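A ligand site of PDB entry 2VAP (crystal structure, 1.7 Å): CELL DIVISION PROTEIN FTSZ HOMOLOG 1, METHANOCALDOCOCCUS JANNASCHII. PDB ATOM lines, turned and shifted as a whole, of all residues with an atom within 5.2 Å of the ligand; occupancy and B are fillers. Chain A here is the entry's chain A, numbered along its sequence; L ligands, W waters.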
ATOM      1  N   CYS A  45     -28.725  13.100  32.127  1.00  0.00           N
ATOM      2  CA  CYS A  45     -27.371  12.620  31.830  1.00  0.00           C
ATOM      3  C   CYS A  45     -26.754  13.339  30.639  1.00  0.00           C
ATOM      4  O   CYS A  45     -27.374  13.448  29.578  1.00  0.00           O
ATOM      5  CB  CYS A  45     -27.410  11.112  31.565  1.00  0.00           C
ATOM      6  SG  CYS A  45     -28.315  10.145  32.787  1.00  0.00           S
ATOM      7  N   GLY A  46     -25.528  13.838  30.819  1.00  0.00           N
ATOM      8  CA  GLY A  46     -24.796  14.502  29.744  1.00  0.00           C
ATOM      9  C   GLY A  46     -25.216  15.946  29.528  1.00  0.00           C
ATOM     10  O   GLY A  46     -26.002  16.489  30.300  1.00  0.00           O
ATOM     11  N   GLY A  47     -24.696  16.550  28.462  1.00  0.00           N
ATOM     12  CA  GLY A  47     -24.949  17.961  28.151  1.00  0.00           C
ATOM     13  C   GLY A  47     -26.422  18.321  28.037  1.00  0.00           C
ATOM     14  O   GLY A  47     -26.919  19.165  28.789  1.00  0.00           O
ATOM     15  N   ALA A  48     -27.109  17.664  27.111  1.00  0.00           N
ATOM     16  CA  ALA A  48     -28.534  17.908  26.883  1.00  0.00           C
ATOM     17  C   ALA A  48     -29.394  17.565  28.097  1.00  0.00           C
ATOM     18  O   ALA A  48     -30.319  18.305  28.437  1.00  0.00           O
ATOM     19  CB  ALA A  48     -29.016  17.145  25.655  1.00  0.00           C
ATOM     20  N   GLY A  49     -29.070  16.442  28.749  1.00  0.00           N
ATOM     21  CA  GLY A  49     -29.759  16.020  29.962  1.00  0.00           C
ATOM     22  C   GLY A  49     -29.623  17.018  31.106  1.00  0.00           C
ATOM     23  O   GLY A  49     -30.586  17.290  31.816  1.00  0.00           O
ATOM     24  N   ASN A  51     -28.985  20.259  30.721  1.00  0.00           N
ATOM     25  CA  ASN A  51     -29.760  21.418  30.290  1.00  0.00           C
ATOM     26  C   ASN A  51     -31.239  21.263  30.604  1.00  0.00           C
ATOM     27  O   ASN A  51     -31.904  22.206  31.041  1.00  0.00           O
ATOM     28  CB  ASN A  51     -29.558  21.659  28.781  1.00  0.00           C
ATOM     29  CG  ASN A  51     -30.105  22.999  28.323  1.00  0.00           C
ATOM     30  OD1 ASN A  51     -29.810  24.046  28.896  1.00  0.00           O
ATOM     31  ND2 ASN A  51     -30.917  22.969  27.272  1.00  0.00           N
ATOM     32  N   ASN A  70     -22.843  14.008  34.926  1.00  0.00           N
ATOM     33  CA  ASN A  70     -22.008  14.315  33.769  1.00  0.00           C
ATOM     34  C   ASN A  70     -20.563  13.912  34.002  1.00  0.00           C
ATOM     35  O   ASN A  70     -20.099  13.856  35.139  1.00  0.00           O
ATOM     36  CB  ASN A  70     -22.081  15.812  33.428  1.00  0.00           C
ATOM     37  CG  ASN A  70     -21.916  16.099  31.945  1.00  0.00           C
ATOM     38  OD1 ASN A  70     -21.167  15.414  31.241  1.00  0.00           O
ATOM     39  ND2 ASN A  70     -22.617  17.113  31.462  1.00  0.00           N
ATOM     40  N   GLN A  75     -19.765  21.610  32.272  1.00  0.00           N
ATOM     41  CA  GLN A  75     -21.202  21.554  32.033  1.00  0.00           C
ATOM     42  C   GLN A  75     -21.976  21.308  33.338  1.00  0.00           C
ATOM     43  O   GLN A  75     -23.034  21.900  33.552  1.00  0.00           O
ATOM     44  CB  GLN A  75     -21.541  20.461  31.002  1.00  0.00           C
ATOM     45  CG  GLN A  75     -20.968  20.710  29.615  1.00  0.00           C
ATOM     46  CD  GLN A  75     -21.390  19.663  28.586  1.00  0.00           C
ATOM     47  OE1 GLN A  75     -21.455  19.952  27.386  1.00  0.00           O
ATOM     48  NE2 GLN A  75     -21.666  18.445  29.039  1.00  0.00           N
ATOM     49  N   ALA A  97     -16.514  13.152  27.810  1.00  0.00           N
ATOM     50  CA  ALA A  97     -16.453  11.823  27.185  1.00  0.00           C
ATOM     51  C   ALA A  97     -16.145  11.880  25.693  1.00  0.00           C
ATOM     52  O   ALA A  97     -15.908  10.839  25.063  1.00  0.00           O
ATOM     53  CB  ALA A  97     -17.750  11.057  27.445  1.00  0.00           C
ATOM     54  N   GLY A  99     -17.907  12.321  23.046  1.00  0.00           N
ATOM     55  CA  GLY A  99     -18.845  11.651  22.145  1.00  0.00           C
ATOM     56  C   GLY A  99     -18.739  10.140  22.095  1.00  0.00           C
ATOM     57  O   GLY A  99     -19.401   9.495  21.282  1.00  0.00           O
ATOM     58  N   GLY A 130     -30.172  13.438  25.699  1.00  0.00           N
ATOM     59  CA  GLY A 130     -30.140  13.381  24.245  1.00  0.00           C
ATOM     60  C   GLY A 130     -29.213  12.246  23.862  1.00  0.00           C
ATOM     61  O   GLY A 130     -28.020  12.278  24.174  1.00  0.00           O
ATOM     62  N   LEU A 131     -29.760  11.226  23.209  1.00  0.00           N
ATOM     63  CA  LEU A 131     -28.951  10.102  22.743  1.00  0.00           C
ATOM     64  C   LEU A 131     -28.150  10.513  21.521  1.00  0.00           C
ATOM     65  O   LEU A 131     -28.609  11.321  20.709  1.00  0.00           O
ATOM     66  CB  LEU A 131     -29.811   8.869  22.444  1.00  0.00           C
ATOM     67  CG  LEU A 131     -30.495   8.153  23.614  1.00  0.00           C
ATOM     68  CD1 LEU A 131     -31.451   7.099  23.088  1.00  0.00           C
ATOM     69  CD2 LEU A 131     -29.482   7.522  24.577  1.00  0.00           C
ATOM     70  N   GLY A 132     -26.938   9.955  21.394  1.00  0.00           N
ATOM     71  CA  GLY A 132     -26.065  10.279  20.266  1.00  0.00           C
ATOM     72  C   GLY A 132     -24.677  10.708  20.686  1.00  0.00           C
ATOM     73  O   GLY A 132     -23.715  10.544  19.937  1.00  0.00           O
ATOM     74  N   GLY A 133     -24.564  11.284  21.888  1.00  0.00           N
ATOM     75  CA  GLY A 133     -23.278  11.720  22.427  1.00  0.00           C
ATOM     76  C   GLY A 133     -22.557  10.614  23.157  1.00  0.00           C
ATOM     77  O   GLY A 133     -22.786   9.428  22.907  1.00  0.00           O
ATOM     78  N   GLY A 134     -21.676  10.993  24.076  1.00  0.00           N
ATOM     79  CA  GLY A 134     -20.900  10.028  24.848  1.00  0.00           C
ATOM     80  C   GLY A 134     -21.448   9.768  26.230  1.00  0.00           C
ATOM     81  O   GLY A 134     -21.736   8.616  26.585  1.00  0.00           O
ATOM     82  N   THR A 135     -21.608  10.830  27.008  1.00  0.00           N
ATOM     83  CA  THR A 135     -22.056  10.727  28.398  1.00  0.00           C
ATOM     84  C   THR A 135     -23.494  10.214  28.506  1.00  0.00           C
ATOM     85  O   THR A 135     -23.749   9.227  29.191  1.00  0.00           O
ATOM     86  CB  THR A 135     -21.899  12.070  29.147  1.00  0.00           C
ATOM     87  OG1 THR A 135     -20.549  12.533  29.022  1.00  0.00           O
ATOM     88  CG2 THR A 135     -22.239  11.928  30.626  1.00  0.00           C
ATOM     89  N   GLY A 136     -24.416  10.881  27.816  1.00  0.00           N
ATOM     90  CA  GLY A 136     -25.827  10.501  27.835  1.00  0.00           C
ATOM     91  C   GLY A 136     -26.055   9.082  27.348  1.00  0.00           C
ATOM     92  O   GLY A 136     -26.616   8.249  28.061  1.00  0.00           O
ATOM     93  N   THR A 137     -25.597   8.803  26.124  1.00  0.00           N
ATOM     94  CA  THR A 137     -25.745   7.484  25.502  1.00  0.00           C
ATOM     95  C   THR A 137     -25.162   6.367  26.364  1.00  0.00           C
ATOM     96  O   THR A 137     -25.754   5.290  26.471  1.00  0.00           O
ATOM     97  CB  THR A 137     -25.081   7.448  24.112  1.00  0.00           C
ATOM     98  OG1 THR A 137     -25.415   8.635  23.372  1.00  0.00           O
ATOM     99  CG2 THR A 137     -25.540   6.233  23.322  1.00  0.00           C
ATOM    100  N   THR A 159     -34.221  11.664  23.471  1.00  0.00           N
ATOM    101  CA  THR A 159     -34.305  12.077  22.073  1.00  0.00           C
ATOM    102  C   THR A 159     -33.322  11.317  21.194  1.00  0.00           C
ATOM    103  O   THR A 159     -32.268  10.880  21.664  1.00  0.00           O
ATOM    104  CB  THR A 159     -34.040  13.591  21.892  1.00  0.00           C
ATOM    105  OG1 THR A 159     -32.717  13.914  22.329  1.00  0.00           O
ATOM    106  CG2 THR A 159     -35.057  14.421  22.668  1.00  0.00           C
ATOM    107  N   LEU A 160     -33.695  11.145  19.931  1.00  0.00           N
ATOM    108  CA  LEU A 160     -32.768  10.692  18.898  1.00  0.00           C
ATOM    109  C   LEU A 160     -32.315  11.924  18.111  1.00  0.00           C
ATOM    110  O   LEU A 160     -33.091  12.857  17.942  1.00  0.00           O
ATOM    111  CB  LEU A 160     -33.431   9.677  17.985  1.00  0.00           C
ATOM    112  CG  LEU A 160     -33.836   8.317  18.582  1.00  0.00           C
ATOM    113  CD1 LEU A 160     -34.624   7.516  17.559  1.00  0.00           C
ATOM    114  CD2 LEU A 160     -32.622   7.528  19.067  1.00  0.00           C
ATOM    115  N   PRO A 161     -31.052  11.918  17.640  1.00  0.00           N
ATOM    116  CA  PRO A 161     -30.475  13.104  16.989  1.00  0.00           C
ATOM    117  C   PRO A 161     -31.120  13.476  15.657  1.00  0.00           C
ATOM    118  O   PRO A 161     -31.794  12.651  15.045  1.00  0.00           O
ATOM    119  CB  PRO A 161     -29.009  12.709  16.776  1.00  0.00           C
ATOM    120  CG  PRO A 161     -29.024  11.231  16.721  1.00  0.00           C
ATOM    121  CD  PRO A 161     -30.083  10.803  17.689  1.00  0.00           C
ATOM    122  N   PHE A 162     -30.905  14.720  15.229  1.00  0.00           N
ATOM    123  CA  PHE A 162     -31.302  15.173  13.898  1.00  0.00           C
ATOM    124  C   PHE A 162     -30.443  14.454  12.859  1.00  0.00           C
ATOM    125  O   PHE A 162     -29.288  14.110  13.128  1.00  0.00           O
ATOM    126  CB  PHE A 162     -31.086  16.681  13.754  1.00  0.00           C
ATOM    127  CG  PHE A 162     -31.934  17.515  14.670  1.00  0.00           C
ATOM    128  CD1 PHE A 162     -33.242  17.854  14.331  1.00  0.00           C
ATOM    129  CD2 PHE A 162     -31.415  17.990  15.872  1.00  0.00           C
ATOM    130  CE1 PHE A 162     -34.023  18.644  15.176  1.00  0.00           C
ATOM    131  CE2 PHE A 162     -32.186  18.781  16.726  1.00  0.00           C
ATOM    132  CZ  PHE A 162     -33.489  19.104  16.372  1.00  0.00           C
ATOM    133  N   GLU A 165     -26.906  15.717  11.995  1.00  0.00           N
ATOM    134  CA  GLU A 165     -25.841  15.446  12.965  1.00  0.00           C
ATOM    135  C   GLU A 165     -24.908  14.335  12.503  1.00  0.00           C
ATOM    136  O   GLU A 165     -23.795  14.194  13.018  1.00  0.00           O
ATOM    137  CB  GLU A 165     -26.417  15.121  14.347  1.00  0.00           C
ATOM    138  CG  GLU A 165     -27.200  16.262  14.988  1.00  0.00           C
ATOM    139  CD  GLU A 165     -27.543  15.986  16.429  1.00  0.00           C
ATOM    140  OE1 GLU A 165     -26.606  15.707  17.209  1.00  0.00           O
ATOM    141  OE2 GLU A 165     -28.738  16.047  16.788  1.00  0.00           O
ATOM    142  N   ARG A 169     -23.505   9.654  14.969  1.00  0.00           N
ATOM    143  CA  ARG A 169     -24.377  10.089  16.063  1.00  0.00           C
ATOM    144  C   ARG A 169     -25.634   9.224  16.171  1.00  0.00           C
ATOM    145  O   ARG A 169     -26.011   8.809  17.266  1.00  0.00           O
ATOM    146  CB  ARG A 169     -24.753  11.565  15.908  1.00  0.00           C
ATOM    147  CG  ARG A 169     -23.644  12.536  16.300  1.00  0.00           C
ATOM    148  CD  ARG A 169     -23.791  13.017  17.738  1.00  0.00           C
ATOM    149  NE  ARG A 169     -22.552  13.596  18.253  1.00  0.00           N
ATOM    150  CZ  ARG A 169     -22.437  14.241  19.407  1.00  0.00           C
ATOM    151  NH1 ARG A 169     -23.491  14.402  20.201  1.00  0.00           N
ATOM    152  NH2 ARG A 169     -21.268  14.729  19.790  1.00  0.00           N
ATOM    153  N   ASN A 192     -35.897  13.793  17.233  1.00  0.00           N
ATOM    154  CA  ASN A 192     -35.666  15.211  16.954  1.00  0.00           C
ATOM    155  C   ASN A 192     -35.891  15.589  15.487  1.00  0.00           C
ATOM    156  O   ASN A 192     -36.329  16.706  15.193  1.00  0.00           O
ATOM    157  CB  ASN A 192     -34.261  15.654  17.384  1.00  0.00           C
ATOM    158  CG  ASN A 192     -34.154  15.914  18.892  1.00  0.00           C
ATOM    159  OD1 ASN A 192     -33.053  16.027  19.431  1.00  0.00           O
ATOM    160  ND2 ASN A 192     -35.297  16.007  19.570  1.00  0.00           N
ATOM    161  N   PHE A 208     -32.396  23.040  18.486  1.00  0.00           N
ATOM    162  CA  PHE A 208     -32.082  22.463  19.793  1.00  0.00           C
ATOM    163  C   PHE A 208     -32.885  23.112  20.922  1.00  0.00           C
ATOM    164  O   PHE A 208     -33.218  22.456  21.907  1.00  0.00           O
ATOM    165  CB  PHE A 208     -30.581  22.559  20.093  1.00  0.00           C
ATOM    166  CG  PHE A 208     -29.735  21.542  19.365  1.00  0.00           C
ATOM    167  CD1 PHE A 208     -30.062  20.188  19.394  1.00  0.00           C
ATOM    168  CD2 PHE A 208     -28.605  21.944  18.670  1.00  0.00           C
ATOM    169  CE1 PHE A 208     -29.288  19.252  18.714  1.00  0.00           C
ATOM    170  CE2 PHE A 208     -27.810  21.013  17.999  1.00  0.00           C
ATOM    171  CZ  PHE A 208     -28.152  19.667  18.022  1.00  0.00           C
ATOM    172  N   ALA A 211     -36.166  21.542  20.752  1.00  0.00           N
ATOM    173  CA  ALA A 211     -35.976  20.233  21.373  1.00  0.00           C
ATOM    174  C   ALA A 211     -35.984  20.323  22.903  1.00  0.00           C
ATOM    175  O   ALA A 211     -36.501  19.427  23.585  1.00  0.00           O
ATOM    176  CB  ALA A 211     -34.681  19.595  20.886  1.00  0.00           C
ATOM    177  N   ASP A 212     -35.416  21.407  23.431  1.00  0.00           N
ATOM    178  CA  ASP A 212     -35.447  21.702  24.864  1.00  0.00           C
ATOM    179  C   ASP A 212     -36.885  21.781  25.388  1.00  0.00           C
ATOM    180  O   ASP A 212     -37.227  21.121  26.373  1.00  0.00           O
ATOM    181  CB  ASP A 212     -34.738  23.019  25.173  1.00  0.00           C
ATOM    182  CG  ASP A 212     -33.230  22.934  25.009  1.00  0.00           C
ATOM    183  OD1 ASP A 212     -32.679  21.806  25.015  1.00  0.00           O
ATOM    184  OD2 ASP A 212     -32.589  23.992  24.880  1.00  0.00           O
ATOM    185  N   LEU A 215     -38.716  18.347  25.322  1.00  0.00           N
ATOM    186  CA  LEU A 215     -38.232  17.524  26.427  1.00  0.00           C
ATOM    187  C   LEU A 215     -38.808  17.959  27.766  1.00  0.00           C
ATOM    188  O   LEU A 215     -39.232  17.120  28.570  1.00  0.00           O
ATOM    189  CB  LEU A 215     -36.702  17.530  26.487  1.00  0.00           C
ATOM    190  CG  LEU A 215     -35.938  16.487  25.662  1.00  0.00           C
ATOM    191  CD1 LEU A 215     -34.463  16.881  25.555  1.00  0.00           C
ATOM    192  CD2 LEU A 215     -36.082  15.093  26.254  1.00  0.00           C
HETATM  193  P1  LIG L   1     -23.120  14.156  25.736  1.00  0.00           P
HETATM  194  O1  LIG L   1     -21.826  13.464  25.403  1.00  0.00           O
HETATM  195  O2  LIG L   1     -22.872  15.236  26.767  1.00  0.00           O
HETATM  196  O3  LIG L   1     -24.095  13.145  26.288  1.00  0.00           O
HETATM  197  O4  LIG L   1     -23.698  14.791  24.378  1.00  0.00           O
HETATM  198  P2  LIG L   1     -24.813  15.950  24.330  1.00  0.00           P
HETATM  199  O5  LIG L   1     -25.818  15.822  25.447  1.00  0.00           O
HETATM  200  O6  LIG L   1     -24.179  17.318  24.309  1.00  0.00           O
HETATM  201  O7  LIG L   1     -25.529  15.667  22.920  1.00  0.00           O
HETATM  202  C1  LIG L   1     -26.126  14.402  22.657  1.00  0.00           C
HETATM  203  C2  LIG L   1     -27.325  14.586  21.740  1.00  0.00           C
HETATM  204  O8  LIG L   1     -28.256  15.495  22.344  1.00  0.00           O
HETATM  205  C3  LIG L   1     -26.919  15.217  20.418  1.00  0.00           C
HETATM  206  O9  LIG L   1     -26.668  14.215  19.422  1.00  0.00           O
HETATM  207  C4  LIG L   1     -28.092  16.110  20.053  1.00  0.00           C
HETATM  208  O10 LIG L   1     -29.038  15.398  19.258  1.00  0.00           O
HETATM  209  C5  LIG L   1     -28.736  16.443  21.390  1.00  0.00           C
HETATM  210  N1  LIG L   1     -28.398  17.825  21.841  1.00  0.00           N
HETATM  211  C6  LIG L   1     -27.195  18.449  21.772  1.00  0.00           C
HETATM  212  N2  LIG L   1     -27.266  19.704  22.289  1.00  0.00           N
HETATM  213  C7  LIG L   1     -28.540  19.895  22.709  1.00  0.00           C
HETATM  214  C8  LIG L   1     -29.304  20.989  23.348  1.00  0.00           C
HETATM  215  O11 LIG L   1     -28.767  22.082  23.635  1.00  0.00           O
HETATM  216  N3  LIG L   1     -30.614  20.778  23.614  1.00  0.00           N
HETATM  217  C9  LIG L   1     -31.230  19.612  23.324  1.00  0.00           C
HETATM  218  N4  LIG L   1     -32.540  19.461  23.614  1.00  0.00           N
HETATM  219  N5  LIG L   1     -30.580  18.572  22.734  1.00  0.00           N
HETATM  220  C10 LIG L   1     -29.268  18.656  22.409  1.00  0.00           C
HETATM  221  O   HOH W   1     -24.474  18.309  19.790  1.00  0.00           O
HETATM  222  O   HOH W   2     -26.846  21.658  25.869  1.00  0.00           O
HETATM  223  O   HOH W   3     -20.751  15.197  28.465  1.00  0.00           O
HETATM  224  O   HOH W   4     -30.209  24.390  23.695  1.00  0.00           O
HETATM  225  O   HOH W   5     -24.801  19.911  24.938  1.00  0.00           O
HETATM  226  O   HOH W   6     -27.624  14.361  27.041  1.00  0.00           O
HETATM  227  O   HOH W   7     -19.221  13.265  25.349  1.00  0.00           O
HETATM  228  O   HOH W   8     -31.805  19.948  26.822  1.00  0.00           O
HETATM  229  O   HOH W   9     -25.083  21.768  20.860  1.00  0.00           O
HETATM  230  O   HOH W  10     -30.557  13.350  20.569  1.00  0.00           O
HETATM  231  O   HOH W  11     -22.940  17.212  21.773  1.00  0.00           O
HETATM  232  O   HOH W  12     -21.033  14.769  22.575  1.00  0.00           O
HETATM  233  O   HOH W  13     -25.530  11.454  24.686  1.00  0.00           O
HETATM  234  O   HOH W  14     -21.781  17.512  25.570  1.00  0.00           O
HETATM  235  O   HOH W  15     -32.503  16.700  22.263  1.00  0.00           O
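Water W7 bridges an oxygen (O1) of the ligand (2.6 Å) and the backbone NH (N) of Gly 99 (2.8 Å). Water W14 bridges an oxygen (O6) of the ligand (2.7 Å) and the side-chain amide oxygen (OE1) of Gln 75 (3.1 Å). Water W15 lies within hydrogen-bond range of a nitrogen (N5) of the ligand (2.7 Å), the side-chain hydroxyl of Thr 159 (2.8 Å) and the side-chain amide oxygen of Asn 192 (3.0 Å). Water W11 lies within hydrogen-bond range of an oxygen (O6) of the ligand (2.8 Å) and the guanidinium group (NH1) of Arg 169 (3.3 Å). Water W12 bridges NH2 of Arg 169 and O1 of the ligand. Water W8 lies within hydrogen-bond range of the side-chain carboxylate (OD1) of Asp 212 (2.7 Å), the backbone carbonyl oxygen (O) of Ala 48 (2.7 Å), the side-chain amide nitrogen (ND2) of Asn 51 (3.2 Å) and a nitrogen (N4) of the ligand (3.3 Å).
N of Phe 162 sits at hydrogen-bond distance from OE2 of Glu 165, 3.0 Å away. The side-chain amide nitrogen of Asn 51 sits at hydrogen-bond distance from the side-chain carboxylate of Asp 212, at 3.1 Å. The backbone carbonyl oxygen of Gly 133 is in hydrogen-bond range of the side-chain hydroxyl of Thr 137, at 2.8 Å. N of Leu 131 is in hydrogen-bond range of O of Thr 159, 3.0 Å away.
Merely in contact with the ligand: Gly 130 (3.2 Å), Ala 211 (3.5 Å), Phe 208 (3.5 Å), Pro 161 (3.5 Å), Gly 133 (3.6 Å), Gly 46 (3.6 Å), Leu 131 (3.7 Å) and Leu 215 (3.8 Å). 16 residues have an atom within 4 Å of the ligand: Gly 46, Gly 47, Ala 48, Gly 130, Leu 131, Gly 133, Gly 134, Thr 135, Gly 136, Pro 161, Glu 165, Arg 169, Phe 208, Ala 211, Asp 212 and Leu 215. The nearest printed residue that does not touch the ligand is Asn 192 (4.1 Å).
O10 of the ligand lies within hydrogen-bond range of OE2 of Glu 165 (2.6 Å). The side-chain carboxylate (OD1) of Asp 212 sits at hydrogen-bond distance from a nitrogen (N3) of the ligand (2.7 Å). N of Gly 136 is in hydrogen-bond range of O3 of the ligand (2.8 Å). N of Ala 48 lies within hydrogen-bond range of O5 of the ligand (2.8 Å). O1 of the ligand lies within hydrogen-bond range of N of Gly 134 (2.8 Å). An oxygen (O2) of the ligand is in hydrogen-bond range of the backbone NH (N) of Gly 47, 2.8 Å away. An oxygen (O1) of the ligand lies within hydrogen-bond range of the backbone NH (N) of Thr 135 (3.1 Å). The guanidinium group of Arg 169 is in hydrogen-bond range of an oxygen (O9) of the ligand (3.3 Å).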
